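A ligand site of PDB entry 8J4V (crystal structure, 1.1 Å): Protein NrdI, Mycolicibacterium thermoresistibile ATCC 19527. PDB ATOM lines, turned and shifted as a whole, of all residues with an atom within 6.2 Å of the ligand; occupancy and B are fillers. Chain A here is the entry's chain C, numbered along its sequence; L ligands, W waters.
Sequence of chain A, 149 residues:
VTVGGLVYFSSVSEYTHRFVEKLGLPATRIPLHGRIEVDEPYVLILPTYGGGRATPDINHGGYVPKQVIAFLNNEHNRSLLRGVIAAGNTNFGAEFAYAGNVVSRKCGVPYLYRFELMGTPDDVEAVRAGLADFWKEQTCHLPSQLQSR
The side-chain hydroxyl (OG) of Ser 13 sits at hydrogen-bond distance from an oxygen (O7) of the ligand (2.5 Å).
The side-chain hydroxyl of Tyr 49 lies within hydrogen-bond range of an oxygen (O9) of the ligand, at 2.6 Å.
An oxygen (O3) of the ligand sits at hydrogen-bond distance from the backbone NH (N) of Thr 48.
An oxygen (O3) of the ligand sits at hydrogen-bond distance from the backbone carbonyl oxygen (O) of Thr 48 (2.7 Å).
The backbone NH of Ser 11 lies within hydrogen-bond range of an oxygen (O9) of the ligand.
An oxygen (O9) of the ligand sits at hydrogen-bond distance from the side-chain hydroxyl (OG) of Ser 11, at 2.7 Å.
OG of Ser 10 is in hydrogen-bond range of O8 of the ligand, at 2.7 Å.
N of Thr 16 is in hydrogen-bond range of O8 of the ligand, 2.9 Å away.
The side-chain hydroxyl of Thr 16 sits at hydrogen-bond distance from an oxygen (O8) of the ligand.
O7 of the ligand lies within hydrogen-bond range of N of Tyr 15 (2.8 Å).
The backbone NH of Ala 97 sits at hydrogen-bond distance from an oxygen (O1) of the ligand.
The backbone carbonyl oxygen (O) of Glu 95 is in hydrogen-bond range of a nitrogen (N2) of the ligand (2.9 Å).
The backbone NH of Gly 51 lies close to an oxygen (O2) of the ligand.
The backbone NH (N) of Asn 89 is in hydrogen-bond range of an oxygen (O1) of the ligand, 2.9 Å away.
O7 of the ligand lies within hydrogen-bond range of N of Glu 14 (3.2 Å).
OH of Tyr 49 sits close to OG of Ser 11.
The backbone NH (N) of Tyr 49 sits at hydrogen-bond distance from the backbone carbonyl oxygen (O) of Tyr 63, at 3.0 Å.
The side-chain hydroxyl of Thr 48 is in hydrogen-bond range of the backbone carbonyl oxygen of Ala 87 (3.0 Å).
OG1 of Thr 48 is in hydrogen-bond range of N of Tyr 98 (3.4 Å).
The side-chain hydroxyl (OG) of Ser 10 lies within hydrogen-bond range of the backbone NH (N) of His 17, 3.0 Å away.
OH of Tyr 63 sits at hydrogen-bond distance from OE2 of Glu 95 (2.5 Å).
OE1 of Glu 95 is in hydrogen-bond range of N of Gly 52, 2.7 Å away.
N of Leu 117 lies within hydrogen-bond range of O of Gly 88 (3.0 Å).
Pro 47 touches the ligand (CB to O6, 3.3 Å).
Gly 50 touches the ligand (N to C5, 3.6 Å).
Tyr 63 touches the ligand.
Ala 87 touches the ligand.
CA of Gly 88 touches O1 of the ligand (3.2 Å).
Phe 92 touches the ligand (CE1 to C12, 3.3 Å).
CA of Phe 96 touches O1 of the ligand, at 3.3 Å.
CA of Leu 117 touches O5 of the ligand (3.4 Å).
Hydrophobic or aromatic side chains within 4 Å of the ligand: Tyr 15, Pro 47, Tyr 49, Tyr 63, Phe 92, Phe 96 and Leu 117.
Within 4 Å of the ligand: Ser 10, Ser 11, Ser 13, Glu 14, Tyr 15, Thr 16, Pro 47, Thr 48, Tyr 49, Gly 50, Gly 51, Tyr 63, Ala 87, Gly 88, Asn 89, Phe 92, Glu 95, Phe 96, Ala 97 and Leu 117.
The nearest printed residue that does not touch the ligand is Phe 9 (4.3 Å).
Water W2 lies within hydrogen-bond range of O5 of the ligand (2.7 Å), O of Leu 117 (2.7 Å) and OG1 of Thr 16 (2.9 Å).
Water W1 bridges an oxygen (O4) of the ligand (2.8 Å) and the side-chain hydroxyl of Ser 13 (3.1 Å).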
ATOM      1  N   PHE A   9       3.857 -19.322  -4.025  1.00  0.00           N
ATOM      2  CA  PHE A   9       4.941 -19.945  -4.776  1.00  0.00           C
ATOM      3  C   PHE A   9       4.329 -20.853  -5.833  1.00  0.00           C
ATOM      4  O   PHE A   9       3.307 -21.502  -5.589  1.00  0.00           O
ATOM      5  CB  PHE A   9       5.873 -20.775  -3.874  1.00  0.00           C
ATOM      6  CG  PHE A   9       6.998 -21.415  -4.629  1.00  0.00           C
ATOM      7  CD1 PHE A   9       8.106 -20.666  -4.999  1.00  0.00           C
ATOM      8  CD2 PHE A   9       6.914 -22.720  -5.050  1.00  0.00           C
ATOM      9  CE1 PHE A   9       9.117 -21.233  -5.741  1.00  0.00           C
ATOM     10  CE2 PHE A   9       7.926 -23.283  -5.801  1.00  0.00           C
ATOM     11  CZ  PHE A   9       9.033 -22.545  -6.143  1.00  0.00           C
ATOM     12  N   SER A  10       4.985 -20.919  -6.994  1.00  0.00           N
ATOM     13  CA  SER A  10       4.564 -21.858  -8.030  1.00  0.00           C
ATOM     14  C   SER A  10       5.805 -22.257  -8.830  1.00  0.00           C
ATOM     15  O   SER A  10       6.618 -21.405  -9.174  1.00  0.00           O
ATOM     16  CB  SER A  10       3.517 -21.193  -8.943  1.00  0.00           C
ATOM     17  OG  SER A  10       2.904 -22.100  -9.847  1.00  0.00           O
ATOM     18  N   SER A  11       5.942 -23.555  -9.104  1.00  0.00           N
ATOM     19  CA  SER A  11       7.073 -24.039  -9.870  1.00  0.00           C
ATOM     20  C   SER A  11       6.785 -23.922 -11.369  1.00  0.00           C
ATOM     21  O   SER A  11       5.814 -23.292 -11.792  1.00  0.00           O
ATOM     22  CB  SER A  11       7.352 -25.503  -9.543  1.00  0.00           C
ATOM     23  OG  SER A  11       6.411 -26.343 -10.211  1.00  0.00           O
ATOM     24  N   VAL A  12       7.623 -24.581 -12.170  1.00  0.00           N
ATOM     25  CA  VAL A  12       7.545 -24.555 -13.630  1.00  0.00           C
ATOM     26  C   VAL A  12       6.212 -25.070 -14.141  1.00  0.00           C
ATOM     27  O   VAL A  12       5.800 -24.727 -15.260  1.00  0.00           O
ATOM     28  CB  VAL A  12       8.752 -25.329 -14.208  1.00  0.00           C
ATOM     29  CG1 VAL A  12       8.561 -26.837 -14.025  1.00  0.00           C
ATOM     30  CG2 VAL A  12       8.965 -24.960 -15.669  1.00  0.00           C
ATOM     31  N   SER A  13       5.520 -25.916 -13.374  1.00  0.00           N
ATOM     32  CA  SER A  13       4.211 -26.391 -13.824  1.00  0.00           C
ATOM     33  C   SER A  13       3.122 -25.330 -13.737  1.00  0.00           C
ATOM     34  O   SER A  13       2.090 -25.459 -14.406  1.00  0.00           O
ATOM     35  CB  SER A  13       3.805 -27.672 -13.092  1.00  0.00           C
ATOM     36  OG  SER A  13       4.096 -27.614 -11.704  1.00  0.00           O
ATOM     37  N   GLU A  14       3.315 -24.291 -12.922  1.00  0.00           N
ATOM     38  CA  GLU A  14       2.468 -23.099 -12.908  1.00  0.00           C
ATOM     39  C   GLU A  14       1.038 -23.342 -12.443  1.00  0.00           C
ATOM     40  O   GLU A  14       0.170 -22.506 -12.698  1.00  0.00           O
ATOM     41  CB  GLU A  14       2.444 -22.374 -14.267  1.00  0.00           C
ATOM     42  CG  GLU A  14       3.822 -22.117 -14.849  1.00  0.00           C
ATOM     43  CD  GLU A  14       4.552 -20.993 -14.139  1.00  0.00           C
ATOM     44  OE1 GLU A  14       3.969 -20.356 -13.245  1.00  0.00           O
ATOM     45  OE2 GLU A  14       5.732 -20.755 -14.470  1.00  0.00           O
ATOM     46  N   TYR A  15       0.759 -24.448 -11.749  1.00  0.00           N
ATOM     47  CA  TYR A  15      -0.617 -24.699 -11.338  1.00  0.00           C
ATOM     48  C   TYR A  15      -1.081 -23.716 -10.271  1.00  0.00           C
ATOM     49  O   TYR A  15      -2.214 -23.222 -10.337  1.00  0.00           O
ATOM     50  CB  TYR A  15      -0.772 -26.133 -10.830  1.00  0.00           C
ATOM     51  CG  TYR A  15      -0.517 -27.187 -11.885  1.00  0.00           C
ATOM     52  CD1 TYR A  15      -0.890 -26.984 -13.212  1.00  0.00           C
ATOM     53  CD2 TYR A  15       0.125 -28.369 -11.560  1.00  0.00           C
ATOM     54  CE1 TYR A  15      -0.643 -27.956 -14.179  1.00  0.00           C
ATOM     55  CE2 TYR A  15       0.381 -29.336 -12.514  1.00  0.00           C
ATOM     56  CZ  TYR A  15      -0.003 -29.127 -13.828  1.00  0.00           C
ATOM     57  OH  TYR A  15       0.242 -30.093 -14.783  1.00  0.00           O
ATOM     58  N   THR A  16      -0.237 -23.429  -9.276  1.00  0.00           N
ATOM     59  CA  THR A  16      -0.628 -22.466  -8.255  1.00  0.00           C
ATOM     60  C   THR A  16      -0.727 -21.070  -8.838  1.00  0.00           C
ATOM     61  O   THR A  16      -1.627 -20.294  -8.480  1.00  0.00           O
ATOM     62  CB  THR A  16       0.374 -22.514  -7.087  1.00  0.00           C
ATOM     63  OG1 THR A  16       0.553 -23.870  -6.667  1.00  0.00           O
ATOM     64  CG2 THR A  16      -0.124 -21.685  -5.912  1.00  0.00           C
ATOM     65  N   HIS A  17       0.182 -20.731  -9.761  1.00  0.00           N
ATOM     66  CA  HIS A  17       0.086 -19.465 -10.475  1.00  0.00           C
ATOM     67  C   HIS A  17      -1.251 -19.331 -11.192  1.00  0.00           C
ATOM     68  O   HIS A  17      -1.907 -18.279 -11.127  1.00  0.00           O
ATOM     69  CB  HIS A  17       1.255 -19.362 -11.448  1.00  0.00           C
ATOM     70  CG  HIS A  17       1.176 -18.176 -12.357  1.00  0.00           C
ATOM     71  ND1 HIS A  17       1.328 -16.877 -11.913  1.00  0.00           N
ATOM     72  CD2 HIS A  17       0.958 -18.100 -13.695  1.00  0.00           C
ATOM     73  CE1 HIS A  17       1.207 -16.055 -12.944  1.00  0.00           C
ATOM     74  NE2 HIS A  17       0.984 -16.768 -14.026  1.00  0.00           N
ATOM     75  N   PRO A  47       2.188 -24.900  -3.017  1.00  0.00           N
ATOM     76  CA  PRO A  47       2.032 -26.318  -3.359  1.00  0.00           C
ATOM     77  C   PRO A  47       2.928 -27.182  -2.484  1.00  0.00           C
ATOM     78  O   PRO A  47       3.772 -26.701  -1.723  1.00  0.00           O
ATOM     79  CB  PRO A  47       2.518 -26.345  -4.818  1.00  0.00           C
ATOM     80  CG  PRO A  47       3.594 -25.318  -4.846  1.00  0.00           C
ATOM     81  CD  PRO A  47       3.155 -24.226  -3.905  1.00  0.00           C
ATOM     82  N   THR A  48       2.744 -28.492  -2.620  1.00  0.00           N
ATOM     83  CA  THR A  48       3.428 -29.500  -1.818  1.00  0.00           C
ATOM     84  C   THR A  48       4.308 -30.328  -2.731  1.00  0.00           C
ATOM     85  O   THR A  48       3.844 -30.837  -3.764  1.00  0.00           O
ATOM     86  CB  THR A  48       2.413 -30.423  -1.146  1.00  0.00           C
ATOM     87  OG1 THR A  48       1.512 -29.632  -0.358  1.00  0.00           O
ATOM     88  CG2 THR A  48       3.112 -31.444  -0.262  1.00  0.00           C
ATOM     89  N   TYR A  49       5.569 -30.504  -2.340  1.00  0.00           N
ATOM     90  CA  TYR A  49       6.448 -31.413  -3.059  1.00  0.00           C
ATOM     91  C   TYR A  49       6.854 -32.534  -2.104  1.00  0.00           C
ATOM     92  O   TYR A  49       6.234 -32.745  -1.056  1.00  0.00           O
ATOM     93  CB  TYR A  49       7.644 -30.656  -3.670  1.00  0.00           C
ATOM     94  CG  TYR A  49       7.239 -29.483  -4.517  1.00  0.00           C
ATOM     95  CD1 TYR A  49       6.204 -29.558  -5.446  1.00  0.00           C
ATOM     96  CD2 TYR A  49       7.875 -28.255  -4.356  1.00  0.00           C
ATOM     97  CE1 TYR A  49       5.823 -28.426  -6.188  1.00  0.00           C
ATOM     98  CE2 TYR A  49       7.514 -27.148  -5.087  1.00  0.00           C
ATOM     99  CZ  TYR A  49       6.489 -27.237  -6.010  1.00  0.00           C
ATOM    100  OH  TYR A  49       6.138 -26.134  -6.730  1.00  0.00           O
ATOM    101  N   GLY A  50       7.875 -33.294  -2.481  1.00  0.00           N
ATOM    102  CA  GLY A  50       8.459 -34.257  -1.568  1.00  0.00           C
ATOM    103  C   GLY A  50       7.645 -35.479  -1.194  1.00  0.00           C
ATOM    104  O   GLY A  50       8.065 -36.233  -0.312  1.00  0.00           O
ATOM    105  N   GLY A  51       6.505 -35.743  -1.839  1.00  0.00           N
ATOM    106  CA  GLY A  51       5.708 -36.888  -1.464  1.00  0.00           C
ATOM    107  C   GLY A  51       6.305 -38.224  -1.847  1.00  0.00           C
ATOM    108  O   GLY A  51       7.247 -38.329  -2.638  1.00  0.00           O
ATOM    109  N   GLY A  52       5.704 -39.280  -1.293  1.00  0.00           N
ATOM    110  CA  GLY A  52       6.110 -40.659  -1.520  1.00  0.00           C
ATOM    111  C   GLY A  52       5.842 -41.578  -0.335  1.00  0.00           C
ATOM    112  O   GLY A  52       5.618 -42.771  -0.522  1.00  0.00           O
ATOM    113  N   TYR A  63       8.320 -31.376   1.920  1.00  0.00           N
ATOM    114  CA  TYR A  63       6.963 -31.017   1.545  1.00  0.00           C
ATOM    115  C   TYR A  63       6.844 -29.532   1.215  1.00  0.00           C
ATOM    116  O   TYR A  63       6.180 -29.157   0.247  1.00  0.00           O
ATOM    117  CB  TYR A  63       5.990 -31.365   2.666  1.00  0.00           C
ATOM    118  CG  TYR A  63       5.905 -32.839   2.913  1.00  0.00           C
ATOM    119  CD1 TYR A  63       5.343 -33.684   1.972  1.00  0.00           C
ATOM    120  CD2 TYR A  63       6.420 -33.400   4.076  1.00  0.00           C
ATOM    121  CE1 TYR A  63       5.276 -35.047   2.190  1.00  0.00           C
ATOM    122  CE2 TYR A  63       6.362 -34.767   4.304  1.00  0.00           C
ATOM    123  CZ  TYR A  63       5.791 -35.587   3.352  1.00  0.00           C
ATOM    124  OH  TYR A  63       5.733 -36.953   3.580  1.00  0.00           O
ATOM    125  N   ALA A  87      -1.820 -26.462  -1.877  1.00  0.00           N
ATOM    126  CA  ALA A  87      -2.207 -27.225  -3.044  1.00  0.00           C
ATOM    127  C   ALA A  87      -1.444 -28.541  -3.083  1.00  0.00           C
ATOM    128  O   ALA A  87      -0.357 -28.683  -2.514  1.00  0.00           O
ATOM    129  CB  ALA A  87      -1.897 -26.437  -4.325  1.00  0.00           C
ATOM    130  N   GLY A  88      -2.039 -29.484  -3.795  1.00  0.00           N
ATOM    131  CA  GLY A  88      -1.426 -30.762  -4.001  1.00  0.00           C
ATOM    132  C   GLY A  88      -2.215 -31.602  -4.985  1.00  0.00           C
ATOM    133  O   GLY A  88      -2.868 -31.071  -5.887  1.00  0.00           O
ATOM    134  N   ASN A  89      -2.152 -32.915  -4.793  1.00  0.00           N
ATOM    135  CA  ASN A  89      -2.784 -33.888  -5.671  1.00  0.00           C
ATOM    136  C   ASN A  89      -3.257 -35.015  -4.771  1.00  0.00           C
ATOM    137  O   ASN A  89      -2.450 -35.596  -4.043  1.00  0.00           O
ATOM    138  CB  ASN A  89      -1.725 -34.360  -6.686  1.00  0.00           C
ATOM    139  CG  ASN A  89      -2.230 -35.419  -7.626  1.00  0.00           C
ATOM    140  OD1 ASN A  89      -3.084 -36.240  -7.282  1.00  0.00           O
ATOM    141  ND2 ASN A  89      -1.722 -35.412  -8.852  1.00  0.00           N
ATOM    142  N   THR A  90      -4.563 -35.297  -4.770  1.00  0.00           N
ATOM    143  CA  THR A  90      -5.093 -36.284  -3.825  1.00  0.00           C
ATOM    144  C   THR A  90      -4.593 -37.698  -4.083  1.00  0.00           C
ATOM    145  O   THR A  90      -4.752 -38.551  -3.201  1.00  0.00           O
ATOM    146  CB  THR A  90      -6.612 -36.289  -3.765  1.00  0.00           C
ATOM    147  OG1 THR A  90      -7.143 -36.593  -5.064  1.00  0.00           O
ATOM    148  CG2 THR A  90      -7.146 -34.940  -3.275  1.00  0.00           C
ATOM    149  N   PHE A  92      -1.758 -38.473  -3.730  1.00  0.00           N
ATOM    150  CA  PHE A  92      -0.787 -38.613  -2.656  1.00  0.00           C
ATOM    151  C   PHE A  92      -1.413 -39.000  -1.314  1.00  0.00           C
ATOM    152  O   PHE A  92      -0.674 -39.198  -0.343  1.00  0.00           O
ATOM    153  CB  PHE A  92       0.048 -37.336  -2.507  1.00  0.00           C
ATOM    154  CG  PHE A  92       1.141 -37.190  -3.543  1.00  0.00           C
ATOM    155  CD1 PHE A  92       0.917 -36.562  -4.748  1.00  0.00           C
ATOM    156  CD2 PHE A  92       2.411 -37.698  -3.290  1.00  0.00           C
ATOM    157  CE1 PHE A  92       1.943 -36.424  -5.694  1.00  0.00           C
ATOM    158  CE2 PHE A  92       3.426 -37.565  -4.227  1.00  0.00           C
ATOM    159  CZ  PHE A  92       3.202 -36.922  -5.415  1.00  0.00           C
ATOM    160  N   GLU A  95      -0.423 -37.738   2.183  1.00  0.00           N
ATOM    161  CA  GLU A  95       0.453 -36.594   1.953  1.00  0.00           C
ATOM    162  C   GLU A  95      -0.225 -35.485   1.172  1.00  0.00           C
ATOM    163  O   GLU A  95       0.447 -34.514   0.782  1.00  0.00           O
ATOM    164  CB  GLU A  95       1.720 -37.049   1.240  1.00  0.00           C
ATOM    165  CG  GLU A  95       2.582 -37.986   2.050  1.00  0.00           C
ATOM    166  CD  GLU A  95       3.728 -38.549   1.242  1.00  0.00           C
ATOM    167  OE1 GLU A  95       3.449 -39.171   0.194  1.00  0.00           O
ATOM    168  OE2 GLU A  95       4.898 -38.407   1.663  1.00  0.00           O
ATOM    169  N   PHE A  96      -1.540 -35.573   0.938  1.00  0.00           N
ATOM    170  CA  PHE A  96      -2.224 -34.564   0.137  1.00  0.00           C
ATOM    171  C   PHE A  96      -2.087 -33.180   0.767  1.00  0.00           C
ATOM    172  O   PHE A  96      -2.515 -32.963   1.908  1.00  0.00           O
ATOM    173  CB  PHE A  96      -3.698 -34.891  -0.011  1.00  0.00           C
ATOM    174  CG  PHE A  96      -4.488 -33.774  -0.644  1.00  0.00           C
ATOM    175  CD1 PHE A  96      -4.096 -33.240  -1.852  1.00  0.00           C
ATOM    176  CD2 PHE A  96      -5.592 -33.217   0.002  1.00  0.00           C
ATOM    177  CE1 PHE A  96      -4.798 -32.188  -2.419  1.00  0.00           C
ATOM    178  CE2 PHE A  96      -6.303 -32.198  -0.569  1.00  0.00           C
ATOM    179  CZ  PHE A  96      -5.901 -31.672  -1.780  1.00  0.00           C
ATOM    180  N   ALA A  97      -1.538 -32.244  -0.003  1.00  0.00           N
ATOM    181  CA  ALA A  97      -1.436 -30.849   0.413  1.00  0.00           C
ATOM    182  C   ALA A  97      -0.702 -30.695   1.737  1.00  0.00           C
ATOM    183  O   ALA A  97      -0.932 -29.734   2.473  1.00  0.00           O
ATOM    184  CB  ALA A  97      -2.800 -30.159   0.415  1.00  0.00           C
ATOM    185  N   TYR A  98       0.216 -31.608   2.028  1.00  0.00           N
ATOM    186  CA  TYR A  98       0.836 -31.672   3.341  1.00  0.00           C
ATOM    187  C   TYR A  98       1.659 -30.436   3.689  1.00  0.00           C
ATOM    188  O   TYR A  98       1.899 -30.186   4.872  1.00  0.00           O
ATOM    189  CB  TYR A  98       1.759 -32.883   3.409  1.00  0.00           C
ATOM    190  CG  TYR A  98       1.863 -33.563   4.749  1.00  0.00           C
ATOM    191  CD1 TYR A  98       0.740 -33.961   5.471  1.00  0.00           C
ATOM    192  CD2 TYR A  98       3.106 -33.811   5.283  1.00  0.00           C
ATOM    193  CE1 TYR A  98       0.872 -34.603   6.698  1.00  0.00           C
ATOM    194  CE2 TYR A  98       3.250 -34.441   6.482  1.00  0.00           C
ATOM    195  CZ  TYR A  98       2.138 -34.844   7.193  1.00  0.00           C
ATOM    196  OH  TYR A  98       2.300 -35.478   8.403  1.00  0.00           O
ATOM    197  N   GLU A 116      -6.604 -28.987  -5.236  1.00  0.00           N
ATOM    198  CA  GLU A 116      -5.795 -29.790  -6.143  1.00  0.00           C
ATOM    199  C   GLU A 116      -5.401 -28.978  -7.365  1.00  0.00           C
ATOM    200  O   GLU A 116      -6.247 -28.333  -7.992  1.00  0.00           O
ATOM    201  CB  GLU A 116      -6.578 -30.995  -6.639  1.00  0.00           C
ATOM    202  CG  GLU A 116      -6.839 -32.066  -5.637  1.00  0.00           C
ATOM    203  CD  GLU A 116      -7.296 -33.331  -6.335  1.00  0.00           C
ATOM    204  OE1 GLU A 116      -6.449 -34.213  -6.600  1.00  0.00           O
ATOM    205  OE2 GLU A 116      -8.483 -33.410  -6.677  1.00  0.00           O
ATOM    206  N   LEU A 117      -4.127 -29.073  -7.742  1.00  0.00           N
ATOM    207  CA  LEU A 117      -3.629 -28.576  -9.025  1.00  0.00           C
ATOM    208  C   LEU A 117      -4.021 -27.113  -9.184  1.00  0.00           C
ATOM    209  O   LEU A 117      -3.746 -26.299  -8.285  1.00  0.00           O
ATOM    210  CB  LEU A 117      -4.065 -29.499 -10.153  1.00  0.00           C
ATOM    211  CG  LEU A 117      -3.702 -30.979 -10.012  1.00  0.00           C
ATOM    212  CD1 LEU A 117      -4.134 -31.713 -11.257  1.00  0.00           C
ATOM    213  CD2 LEU A 117      -2.218 -31.135  -9.795  1.00  0.00           C
ATOM    214  N   MET A 118      -4.654 -26.730 -10.299  1.00  0.00           N
ATOM    215  CA  MET A 118      -4.987 -25.343 -10.552  1.00  0.00           C
ATOM    216  C   MET A 118      -6.325 -24.946  -9.944  1.00  0.00           C
ATOM    217  O   MET A 118      -6.755 -23.808 -10.134  1.00  0.00           O
ATOM    218  CB  MET A 118      -5.039 -25.059 -12.054  1.00  0.00           C
ATOM    219  CG  MET A 118      -6.093 -25.826 -12.861  1.00  0.00           C
ATOM    220  SD  MET A 118      -5.971 -27.618 -13.018  1.00  0.00           S
ATOM    221  CE  MET A 118      -4.393 -27.791 -13.844  1.00  0.00           C
HETATM  222  N1  LIG L   1       1.068 -33.195  -3.982  1.00  0.00           N
HETATM  223  C1  LIG L   1       0.658 -33.544  -2.729  1.00  0.00           C
HETATM  224  O1  LIG L   1      -0.514 -33.359  -2.396  1.00  0.00           O
HETATM  225  N2  LIG L   1       1.554 -34.098  -1.844  1.00  0.00           N
HETATM  226  C2  LIG L   1       2.860 -34.356  -2.190  1.00  0.00           C
HETATM  227  O2  LIG L   1       3.596 -34.875  -1.333  1.00  0.00           O
HETATM  228  C3  LIG L   1       3.292 -34.018  -3.467  1.00  0.00           C
HETATM  229  N3  LIG L   1       4.591 -34.240  -3.874  1.00  0.00           N
HETATM  230  C4  LIG L   1       4.973 -33.899  -5.164  1.00  0.00           C
HETATM  231  C5  LIG L   1       6.283 -34.143  -5.568  1.00  0.00           C
HETATM  232  C6  LIG L   1       6.714 -33.796  -6.841  1.00  0.00           C
HETATM  233  C7  LIG L   1       8.136 -34.044  -7.274  1.00  0.00           C
HETATM  234  C8  LIG L   1       5.807 -33.211  -7.725  1.00  0.00           C
HETATM  235  C9  LIG L   1       6.236 -32.827  -9.113  1.00  0.00           C
HETATM  236  C10 LIG L   1       4.488 -32.971  -7.312  1.00  0.00           C
HETATM  237  C11 LIG L   1       4.056 -33.318  -6.038  1.00  0.00           C
HETATM  238  N4  LIG L   1       2.756 -33.068  -5.620  1.00  0.00           N
HETATM  239  C12 LIG L   1       2.375 -33.433  -4.351  1.00  0.00           C
HETATM  240  C13 LIG L   1       1.759 -32.420  -6.537  1.00  0.00           C
HETATM  241  C14 LIG L   1       1.951 -30.899  -6.595  1.00  0.00           C
HETATM  242  O3  LIG L   1       1.763 -30.300  -5.323  1.00  0.00           O
HETATM  243  C15 LIG L   1       0.908 -30.304  -7.547  1.00  0.00           C
HETATM  244  O4  LIG L   1       1.166 -30.771  -8.867  1.00  0.00           O
HETATM  245  C16 LIG L   1       0.843 -28.783  -7.512  1.00  0.00           C
HETATM  246  O5  LIG L   1      -0.300 -28.394  -8.241  1.00  0.00           O
HETATM  247  C17 LIG L   1       2.090 -28.150  -8.106  1.00  0.00           C
HETATM  248  O6  LIG L   1       1.972 -26.737  -8.000  1.00  0.00           O
HETATM  249  P1  LIG L   1       2.863 -25.781  -8.926  1.00  0.00           P
HETATM  250  O7  LIG L   1       2.564 -26.121 -10.367  1.00  0.00           O
HETATM  251  O8  LIG L   1       2.389 -24.400  -8.582  1.00  0.00           O
HETATM  252  O9  LIG L   1       4.321 -26.015  -8.601  1.00  0.00           O
HETATM  253  O   HOH W   1       3.564 -30.328 -10.332  1.00  0.00           O
HETATM  254  O   HOH W   2      -1.182 -26.022  -7.366  1.00  0.00           O
